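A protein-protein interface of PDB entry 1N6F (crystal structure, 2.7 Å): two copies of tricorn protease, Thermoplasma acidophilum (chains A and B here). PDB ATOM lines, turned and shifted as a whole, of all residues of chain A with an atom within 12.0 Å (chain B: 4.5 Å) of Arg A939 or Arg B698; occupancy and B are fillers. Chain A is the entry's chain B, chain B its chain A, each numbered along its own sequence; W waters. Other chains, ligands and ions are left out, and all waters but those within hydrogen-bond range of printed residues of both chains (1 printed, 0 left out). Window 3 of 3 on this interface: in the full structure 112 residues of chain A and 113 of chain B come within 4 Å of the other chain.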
ATOM      1  N   TYR A 935      15.968  -3.955   8.358  1.00  0.00           N
ATOM      2  CA  TYR A 935      15.140  -3.377   9.396  1.00  0.00           C
ATOM      3  C   TYR A 935      15.996  -2.741  10.472  1.00  0.00           C
ATOM      4  O   TYR A 935      17.180  -3.033  10.617  1.00  0.00           O
ATOM      5  CB  TYR A 935      14.250  -4.433  10.050  1.00  0.00           C
ATOM      6  CG  TYR A 935      13.036  -4.810   9.258  1.00  0.00           C
ATOM      7  CD1 TYR A 935      13.012  -5.980   8.483  1.00  0.00           C
ATOM      8  CD2 TYR A 935      11.885  -4.010   9.297  1.00  0.00           C
ATOM      9  CE1 TYR A 935      11.863  -6.351   7.760  1.00  0.00           C
ATOM     10  CE2 TYR A 935      10.730  -4.372   8.578  1.00  0.00           C
ATOM     11  CZ  TYR A 935      10.731  -5.551   7.807  1.00  0.00           C
ATOM     12  OH  TYR A 935       9.604  -5.893   7.080  1.00  0.00           O
ATOM     13  N   ASP A 936      15.357  -1.881  11.243  1.00  0.00           N
ATOM     14  CA  ASP A 936      16.013  -1.169  12.317  1.00  0.00           C
ATOM     15  C   ASP A 936      15.454  -1.685  13.644  1.00  0.00           C
ATOM     16  O   ASP A 936      14.246  -1.711  13.838  1.00  0.00           O
ATOM     17  CB  ASP A 936      15.737   0.325  12.130  1.00  0.00           C
ATOM     18  CG  ASP A 936      16.457   1.191  13.131  1.00  0.00           C
ATOM     19  OD1 ASP A 936      16.456   2.432  12.910  1.00  0.00           O
ATOM     20  OD2 ASP A 936      17.002   0.644  14.125  1.00  0.00           O
ATOM     21  N   ASN A 937      16.330  -2.113  14.546  1.00  0.00           N
ATOM     22  CA  ASN A 937      15.891  -2.613  15.840  1.00  0.00           C
ATOM     23  C   ASN A 937      16.133  -1.692  16.981  1.00  0.00           C
ATOM     24  O   ASN A 937      17.256  -1.545  17.450  1.00  0.00           O
ATOM     25  CB  ASN A 937      16.552  -3.918  16.173  1.00  0.00           C
ATOM     26  CG  ASN A 937      15.672  -5.063  15.863  1.00  0.00           C
ATOM     27  OD1 ASN A 937      15.439  -5.357  14.694  1.00  0.00           O
ATOM     28  ND2 ASN A 937      15.137  -5.710  16.902  1.00  0.00           N
ATOM     29  N   PRO A 938      15.066  -1.077  17.472  1.00  0.00           N
ATOM     30  CA  PRO A 938      15.192  -0.153  18.590  1.00  0.00           C
ATOM     31  C   PRO A 938      15.064  -0.840  19.933  1.00  0.00           C
ATOM     32  O   PRO A 938      14.348  -1.841  20.068  1.00  0.00           O
ATOM     33  CB  PRO A 938      14.051   0.821  18.350  1.00  0.00           C
ATOM     34  CG  PRO A 938      12.985  -0.072  17.822  1.00  0.00           C
ATOM     35  CD  PRO A 938      13.727  -0.987  16.869  1.00  0.00           C
ATOM     36  N   ARG A 939      15.773  -0.305  20.922  1.00  0.00           N
ATOM     37  CA  ARG A 939      15.709  -0.852  22.262  1.00  0.00           C
ATOM     38  C   ARG A 939      14.233  -0.887  22.642  1.00  0.00           C
ATOM     39  O   ARG A 939      13.730  -1.896  23.113  1.00  0.00           O
ATOM     40  CB  ARG A 939      16.486   0.039  23.229  1.00  0.00           C
ATOM     41  CG  ARG A 939      16.280  -0.287  24.696  1.00  0.00           C
ATOM     42  CD  ARG A 939      16.614  -1.736  25.043  1.00  0.00           C
ATOM     43  NE  ARG A 939      16.562  -1.943  26.493  1.00  0.00           N
ATOM     44  CZ  ARG A 939      17.474  -1.482  27.343  1.00  0.00           C
ATOM     45  NH1 ARG A 939      17.338  -1.710  28.629  1.00  0.00           N
ATOM     46  NH2 ARG A 939      18.525  -0.811  26.904  1.00  0.00           N
ATOM     47  N   ARG A 940      13.543   0.224  22.421  1.00  0.00           N
ATOM     48  CA  ARG A 940      12.128   0.298  22.732  1.00  0.00           C
ATOM     49  C   ARG A 940      11.360   0.797  21.521  1.00  0.00           C
ATOM     50  O   ARG A 940      11.692   1.832  20.945  1.00  0.00           O
ATOM     51  CB  ARG A 940      11.886   1.210  23.927  1.00  0.00           C
ATOM     52  CG  ARG A 940      12.517   2.567  23.805  1.00  0.00           C
ATOM     53  CD  ARG A 940      12.353   3.380  25.110  1.00  0.00           C
ATOM     54  NE  ARG A 940      12.999   2.729  26.252  1.00  0.00           N
ATOM     55  CZ  ARG A 940      14.298   2.787  26.516  1.00  0.00           C
ATOM     56  NH1 ARG A 940      14.780   2.138  27.568  1.00  0.00           N
ATOM     57  NH2 ARG A 940      15.105   3.507  25.744  1.00  0.00           N
ATOM     58  N   GLY A 941      10.338   0.045  21.126  1.00  0.00           N
ATOM     59  CA  GLY A 941       9.554   0.410  19.964  1.00  0.00           C
ATOM     60  C   GLY A 941       9.454  -0.763  19.008  1.00  0.00           C
ATOM     61  O   GLY A 941       9.851  -1.887  19.325  1.00  0.00           O
ATOM     62  N   THR A 942       8.926  -0.499  17.825  1.00  0.00           N
ATOM     63  CA  THR A 942       8.762  -1.540  16.836  1.00  0.00           C
ATOM     64  C   THR A 942       9.765  -1.399  15.702  1.00  0.00           C
ATOM     65  O   THR A 942      10.440  -0.373  15.576  1.00  0.00           O
ATOM     66  CB  THR A 942       7.349  -1.512  16.263  1.00  0.00           C
ATOM     67  OG1 THR A 942       7.112  -0.251  15.634  1.00  0.00           O
ATOM     68  CG2 THR A 942       6.335  -1.683  17.371  1.00  0.00           C
ATOM     69  N   LEU A 943       9.853  -2.445  14.880  1.00  0.00           N
ATOM     70  CA  LEU A 943      10.756  -2.470  13.748  1.00  0.00           C
ATOM     71  C   LEU A 943      10.507  -1.327  12.798  1.00  0.00           C
ATOM     72  O   LEU A 943       9.382  -0.848  12.627  1.00  0.00           O
ATOM     73  CB  LEU A 943      10.583  -3.759  12.964  1.00  0.00           C
ATOM     74  CG  LEU A 943      10.981  -5.042  13.668  1.00  0.00           C
ATOM     75  CD1 LEU A 943      10.600  -6.214  12.774  1.00  0.00           C
ATOM     76  CD2 LEU A 943      12.478  -5.036  13.948  1.00  0.00           C
ATOM     77  N   SER A 944      11.567  -0.899  12.150  1.00  0.00           N
ATOM     78  CA  SER A 944      11.441   0.171  11.180  1.00  0.00           C
ATOM     79  C   SER A 944      12.031  -0.345   9.864  1.00  0.00           C
ATOM     80  O   SER A 944      13.235  -0.583   9.774  1.00  0.00           O
ATOM     81  CB  SER A 944      12.194   1.394  11.705  1.00  0.00           C
ATOM     82  OG  SER A 944      11.630   2.559  11.172  1.00  0.00           O
ATOM     83  N   TRP B 694      26.188   6.534  32.800  1.00  0.00           N
ATOM     84  CA  TRP B 694      26.139   5.101  32.974  1.00  0.00           C
ATOM     85  C   TRP B 694      24.700   4.612  32.854  1.00  0.00           C
ATOM     86  O   TRP B 694      24.438   3.613  32.200  1.00  0.00           O
ATOM     87  CB  TRP B 694      26.708   4.720  34.338  1.00  0.00           C
ATOM     88  CG  TRP B 694      26.572   3.262  34.693  1.00  0.00           C
ATOM     89  CD1 TRP B 694      27.469   2.283  34.458  1.00  0.00           C
ATOM     90  CD2 TRP B 694      25.456   2.643  35.348  1.00  0.00           C
ATOM     91  NE1 TRP B 694      26.987   1.086  34.916  1.00  0.00           N
ATOM     92  CE2 TRP B 694      25.750   1.275  35.462  1.00  0.00           C
ATOM     93  CE3 TRP B 694      24.229   3.116  35.831  1.00  0.00           C
ATOM     94  CZ2 TRP B 694      24.892   0.375  36.062  1.00  0.00           C
ATOM     95  CZ3 TRP B 694      23.369   2.227  36.424  1.00  0.00           C
ATOM     96  CH2 TRP B 694      23.703   0.858  36.528  1.00  0.00           C
ATOM     97  N   LYS B 695      23.758   5.317  33.466  1.00  0.00           N
ATOM     98  CA  LYS B 695      22.350   4.904  33.398  1.00  0.00           C
ATOM     99  C   LYS B 695      21.768   4.969  31.994  1.00  0.00           C
ATOM    100  O   LYS B 695      20.978   4.110  31.598  1.00  0.00           O
ATOM    101  CB  LYS B 695      21.490   5.748  34.343  1.00  0.00           C
ATOM    102  CG  LYS B 695      20.065   5.248  34.486  1.00  0.00           C
ATOM    103  CD  LYS B 695      19.209   6.295  35.189  1.00  0.00           C
ATOM    104  CE  LYS B 695      17.727   5.914  35.198  1.00  0.00           C
ATOM    105  NZ  LYS B 695      17.507   4.639  35.949  1.00  0.00           N
ATOM    106  N   LEU B 696      22.158   5.990  31.240  1.00  0.00           N
ATOM    107  CA  LEU B 696      21.694   6.145  29.853  1.00  0.00           C
ATOM    108  C   LEU B 696      22.256   5.034  28.955  1.00  0.00           C
ATOM    109  O   LEU B 696      21.578   4.470  28.124  1.00  0.00           O
ATOM    110  CB  LEU B 696      22.117   7.529  29.300  1.00  0.00           C
ATOM    111  CG  LEU B 696      21.379   8.754  29.864  1.00  0.00           C
ATOM    112  CD1 LEU B 696      22.006  10.006  29.377  1.00  0.00           C
ATOM    113  CD2 LEU B 696      19.923   8.693  29.462  1.00  0.00           C
ATOM    114  N   ALA B 697      23.525   4.731  29.148  1.00  0.00           N
ATOM    115  CA  ALA B 697      24.183   3.714  28.353  1.00  0.00           C
ATOM    116  C   ALA B 697      23.469   2.385  28.507  1.00  0.00           C
ATOM    117  O   ALA B 697      23.363   1.607  27.555  1.00  0.00           O
ATOM    118  CB  ALA B 697      25.635   3.575  28.761  1.00  0.00           C
ATOM    119  N   ARG B 698      22.965   2.125  29.704  1.00  0.00           N
ATOM    120  CA  ARG B 698      22.267   0.877  29.951  1.00  0.00           C
ATOM    121  C   ARG B 698      20.821   0.929  29.481  1.00  0.00           C
ATOM    122  O   ARG B 698      20.330  -0.012  28.858  1.00  0.00           O
ATOM    123  CB  ARG B 698      22.283   0.546  31.432  1.00  0.00           C
ATOM    124  CG  ARG B 698      21.700  -0.793  31.713  1.00  0.00           C
ATOM    125  CD  ARG B 698      21.341  -0.851  33.156  1.00  0.00           C
ATOM    126  NE  ARG B 698      20.459   0.256  33.502  1.00  0.00           N
ATOM    127  CZ  ARG B 698      19.928   0.405  34.708  1.00  0.00           C
ATOM    128  NH1 ARG B 698      19.135   1.447  34.959  1.00  0.00           N
ATOM    129  NH2 ARG B 698      20.200  -0.499  35.663  1.00  0.00           N
ATOM    130  N   ASP B 699      20.144   2.030  29.783  1.00  0.00           N
ATOM    131  CA  ASP B 699      18.755   2.170  29.399  1.00  0.00           C
ATOM    132  C   ASP B 699      18.525   2.345  27.895  1.00  0.00           C
ATOM    133  O   ASP B 699      17.437   2.094  27.403  1.00  0.00           O
ATOM    134  CB  ASP B 699      18.129   3.325  30.181  1.00  0.00           C
ATOM    135  CG  ASP B 699      17.947   3.001  31.656  1.00  0.00           C
ATOM    136  OD1 ASP B 699      17.638   3.924  32.454  1.00  0.00           O
ATOM    137  OD2 ASP B 699      18.118   1.815  32.009  1.00  0.00           O
ATOM    138  N   ASN B 700      19.542   2.750  27.153  1.00  0.00           N
ATOM    139  CA  ASN B 700      19.344   2.942  25.732  1.00  0.00           C
ATOM    140  C   ASN B 700      20.043   1.955  24.797  1.00  0.00           C
ATOM    141  O   ASN B 700      19.832   2.000  23.580  1.00  0.00           O
ATOM    142  CB  ASN B 700      19.716   4.379  25.325  1.00  0.00           C
ATOM    143  CG  ASN B 700      18.867   5.426  26.015  1.00  0.00           C
ATOM    144  OD1 ASN B 700      17.671   5.233  26.221  1.00  0.00           O
ATOM    145  ND2 ASN B 700      19.484   6.548  26.374  1.00  0.00           N
ATOM    146  N   TYR B 701      20.873   1.071  25.344  1.00  0.00           N
ATOM    147  CA  TYR B 701      21.568   0.086  24.515  1.00  0.00           C
ATOM    148  C   TYR B 701      20.534  -0.717  23.721  1.00  0.00           C
ATOM    149  O   TYR B 701      19.507  -1.139  24.248  1.00  0.00           O
ATOM    150  CB  TYR B 701      22.402  -0.863  25.378  1.00  0.00           C
ATOM    151  CG  TYR B 701      23.375  -1.693  24.573  1.00  0.00           C
ATOM    152  CD1 TYR B 701      24.471  -1.104  23.956  1.00  0.00           C
ATOM    153  CD2 TYR B 701      23.165  -3.063  24.371  1.00  0.00           C
ATOM    154  CE1 TYR B 701      25.337  -1.856  23.152  1.00  0.00           C
ATOM    155  CE2 TYR B 701      24.020  -3.817  23.559  1.00  0.00           C
ATOM    156  CZ  TYR B 701      25.103  -3.203  22.952  1.00  0.00           C
ATOM    157  OH  TYR B 701      25.924  -3.929  22.116  1.00  0.00           O
ATOM    158  N   TRP B 702      20.808  -0.931  22.447  1.00  0.00           N
ATOM    159  CA  TRP B 702      19.868  -1.648  21.608  1.00  0.00           C
ATOM    160  C   TRP B 702      19.457  -3.012  22.154  1.00  0.00           C
ATOM    161  O   TRP B 702      18.294  -3.396  22.092  1.00  0.00           O
ATOM    162  CB  TRP B 702      20.434  -1.802  20.191  1.00  0.00           C
ATOM    163  CG  TRP B 702      21.587  -2.732  20.104  1.00  0.00           C
ATOM    164  CD1 TRP B 702      22.889  -2.475  20.445  1.00  0.00           C
ATOM    165  CD2 TRP B 702      21.546  -4.085  19.662  1.00  0.00           C
ATOM    166  NE1 TRP B 702      23.663  -3.588  20.241  1.00  0.00           N
ATOM    167  CE2 TRP B 702      22.864  -4.596  19.769  1.00  0.00           C
ATOM    168  CE3 TRP B 702      20.523  -4.924  19.190  1.00  0.00           C
ATOM    169  CZ2 TRP B 702      23.182  -5.901  19.419  1.00  0.00           C
ATOM    170  CZ3 TRP B 702      20.840  -6.221  18.838  1.00  0.00           C
ATOM    171  CH2 TRP B 702      22.158  -6.701  18.960  1.00  0.00           C
ATOM    172  N   GLU B 704      18.638  -5.040  25.145  1.00  0.00           N
ATOM    173  CA  GLU B 704      18.242  -5.003  26.553  1.00  0.00           C
ATOM    174  C   GLU B 704      18.890  -6.076  27.420  1.00  0.00           C
ATOM    175  O   GLU B 704      19.314  -5.808  28.552  1.00  0.00           O
ATOM    176  CB  GLU B 704      16.734  -5.122  26.653  1.00  0.00           C
ATOM    177  CG  GLU B 704      16.221  -5.114  28.059  1.00  0.00           C
ATOM    178  CD  GLU B 704      14.711  -5.151  28.102  1.00  0.00           C
ATOM    179  OE1 GLU B 704      14.151  -5.296  29.212  1.00  0.00           O
ATOM    180  OE2 GLU B 704      14.081  -5.034  27.026  1.00  0.00           O
ATOM    181  N   ALA B 707      22.594  -5.385  28.209  1.00  0.00           N
ATOM    182  CA  ALA B 707      22.693  -4.199  29.061  1.00  0.00           C
ATOM    183  C   ALA B 707      22.799  -4.530  30.551  1.00  0.00           C
ATOM    184  O   ALA B 707      23.736  -4.085  31.233  1.00  0.00           O
ATOM    185  CB  ALA B 707      21.504  -3.295  28.822  1.00  0.00           C
ATOM    186  N   SER B 711      26.221  -3.292  32.119  1.00  0.00           N
ATOM    187  CA  SER B 711      26.113  -2.189  33.049  1.00  0.00           C
ATOM    188  C   SER B 711      26.612  -2.553  34.434  1.00  0.00           C
ATOM    189  O   SER B 711      27.540  -1.936  34.951  1.00  0.00           O
ATOM    190  CB  SER B 711      24.667  -1.747  33.141  1.00  0.00           C
ATOM    191  OG  SER B 711      23.873  -2.831  33.544  1.00  0.00           O
ATOM    192  N   TYR B 742      30.660  -1.231  26.156  1.00  0.00           N
ATOM    193  CA  TYR B 742      29.552  -1.838  25.428  1.00  0.00           C
ATOM    194  C   TYR B 742      30.034  -2.421  24.106  1.00  0.00           C
ATOM    195  O   TYR B 742      29.247  -2.975  23.345  1.00  0.00           O
ATOM    196  CB  TYR B 742      28.395  -0.847  25.187  1.00  0.00           C
ATOM    197  CG  TYR B 742      27.560  -0.603  26.430  1.00  0.00           C
ATOM    198  CD1 TYR B 742      27.924   0.369  27.370  1.00  0.00           C
ATOM    199  CD2 TYR B 742      26.444  -1.404  26.711  1.00  0.00           C
ATOM    200  CE1 TYR B 742      27.195   0.526  28.564  1.00  0.00           C
ATOM    201  CE2 TYR B 742      25.712  -1.252  27.900  1.00  0.00           C
ATOM    202  CZ  TYR B 742      26.097  -0.289  28.825  1.00  0.00           C
ATOM    203  OH  TYR B 742      25.426  -0.163  30.012  1.00  0.00           O
ATOM    204  N   GLU B1010      21.348   2.884  20.203  1.00  0.00           N
ATOM    205  CA  GLU B1010      19.969   2.462  20.473  1.00  0.00           C
ATOM    206  C   GLU B1010      19.212   1.830  19.309  1.00  0.00           C
ATOM    207  O   GLU B1010      18.200   1.153  19.520  1.00  0.00           O
ATOM    208  CB  GLU B1010      19.182   3.680  20.956  1.00  0.00           C
ATOM    209  CG  GLU B1010      17.882   3.392  21.669  1.00  0.00           C
ATOM    210  CD  GLU B1010      17.268   4.652  22.272  1.00  0.00           C
ATOM    211  OE1 GLU B1010      18.022   5.600  22.538  1.00  0.00           O
ATOM    212  OE2 GLU B1010      16.041   4.690  22.482  1.00  0.00           O
HETATM  213  O   HOH W   1      14.843  -2.624  30.329  1.00  0.00           O
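The backbone carbonyl oxygen of Arg B698 lies within hydrogen-bond range of the guanidinium group of Arg A939. The backbone carbonyl oxygen (O) of Asp B699 sits at hydrogen-bond distance from the guanidinium group (NH2) of Arg A939 (3.1 Å). The guanidinium group (NH1) of Arg A940 sits at hydrogen-bond distance from the backbone carbonyl oxygen (O) of Asp B699 (2.7 Å). The side-chain amide oxygen (OD1) of Asn B700 is in hydrogen-bond range of the guanidinium group (NH2) of Arg A940 (3.1 Å). The guanidinium group (NH2) of Arg A939 is in hydrogen-bond range of the backbone carbonyl oxygen (O) of Tyr B701 (2.9 Å). OE2 of Glu B704 is in salt-bridge range of NE of Arg A939. The backbone NH (N) of Arg A939 sits at hydrogen-bond distance from the backbone carbonyl oxygen (O) of Glu B1010 (3.2 Å). The side-chain carboxylate (OE2) of Glu B1010 lies within salt-bridge range of the guanidinium group (NH2) of Arg A940 (3.6 Å).
The side-chain amino group (NZ) of Lys B695 lies within salt-bridge range of the side-chain carboxylate (OD1) of Asp B699 (3.6 Å). The backbone carbonyl oxygen (O) of Leu B696 lies close to the side-chain amide nitrogen (ND2) of Asn B700, 3.4 Å away. The side-chain carboxylate (OD2) of Asp B699 is in salt-bridge range of the guanidinium group (NH1) of Arg B698. The side-chain hydroxyl of Tyr B742 lies close to the backbone NH of Arg B698, 3.4 Å away. The indole nitrogen (NE1) of Trp B702 sits at hydrogen-bond distance from the side-chain hydroxyl (OH) of Tyr B701 (3.0 Å).
O of Asn A937 touches O of Glu B1010, 3.5 Å away. CA of Pro A938 touches O of Glu B1010, at 3.4 Å. NH2 of Arg A939 touches N of Asn B700, 3.7 Å away. Trp B702 touches Arg A939 (O to CA, 3.6 Å).
Printed residues of chain B within 4 Å of Arg A939: Arg B698 (2.8 Å), Asp B699 (3.1 Å), Asn B700 (3.7 Å), Tyr B701 (2.9 Å), Trp B702 (3.6 Å), Glu B704 (3.2 Å) and Glu B1010 (3.2 Å). Of chain A, only Arg A939 comes within 4 Å of Arg B698. Lys B695 touches none of the printed residues of chain A. No residue of chain A comes within 4 Å of Leu B696. No residue of chain A comes within 4 Å of Ala B697. Of chain A, only Arg A939 and Arg A940 come within 4 Å of Asp B699. No residue of chain A comes within 4 Å of Ala B707. Ser B711 touches none of the printed residues of chain A. Of chain A, only Asn A937 (3.5 Å), Pro A938 (3.4 Å), Arg A939 (3.2 Å) and Arg A940 (3.6 Å) come within 4 Å of Glu B1010. Of the printed residues of chain B, Asn A937 touches Glu B1010 (3.5 Å). Of the printed residues of chain B, Pro A938 touches Glu B1010. Printed residues of chain B within 4 Å of Arg A940: Asp B699, Asn B700 and Glu B1010. Printed residues of chain A within 4 Å of Tyr B701: Arg A939. Printed residues of chain A within 4 Å of Trp B702: Arg A939. Gly A941 touches none of the printed residues of chain B.
Of the 14 printed residues of chain B, 7 touch a printed residue of chain A. Printed residues of chain B that touch a printed residue of chain A: Arg B698, Asp B699, Asn B700, Tyr B701, Trp B702, Glu B704 and Glu B1010. Among the printed residues, 12 pairs touch across the chains.
No position is printed for both chains. Of the 12 pairs that touch across the chains among the printed residues, none has its exchanged pair printed and touching as well.
Water W1 bridges OE1 of Glu B704 (3.0 Å) and NH1 of Arg A939 (3.2 Å).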
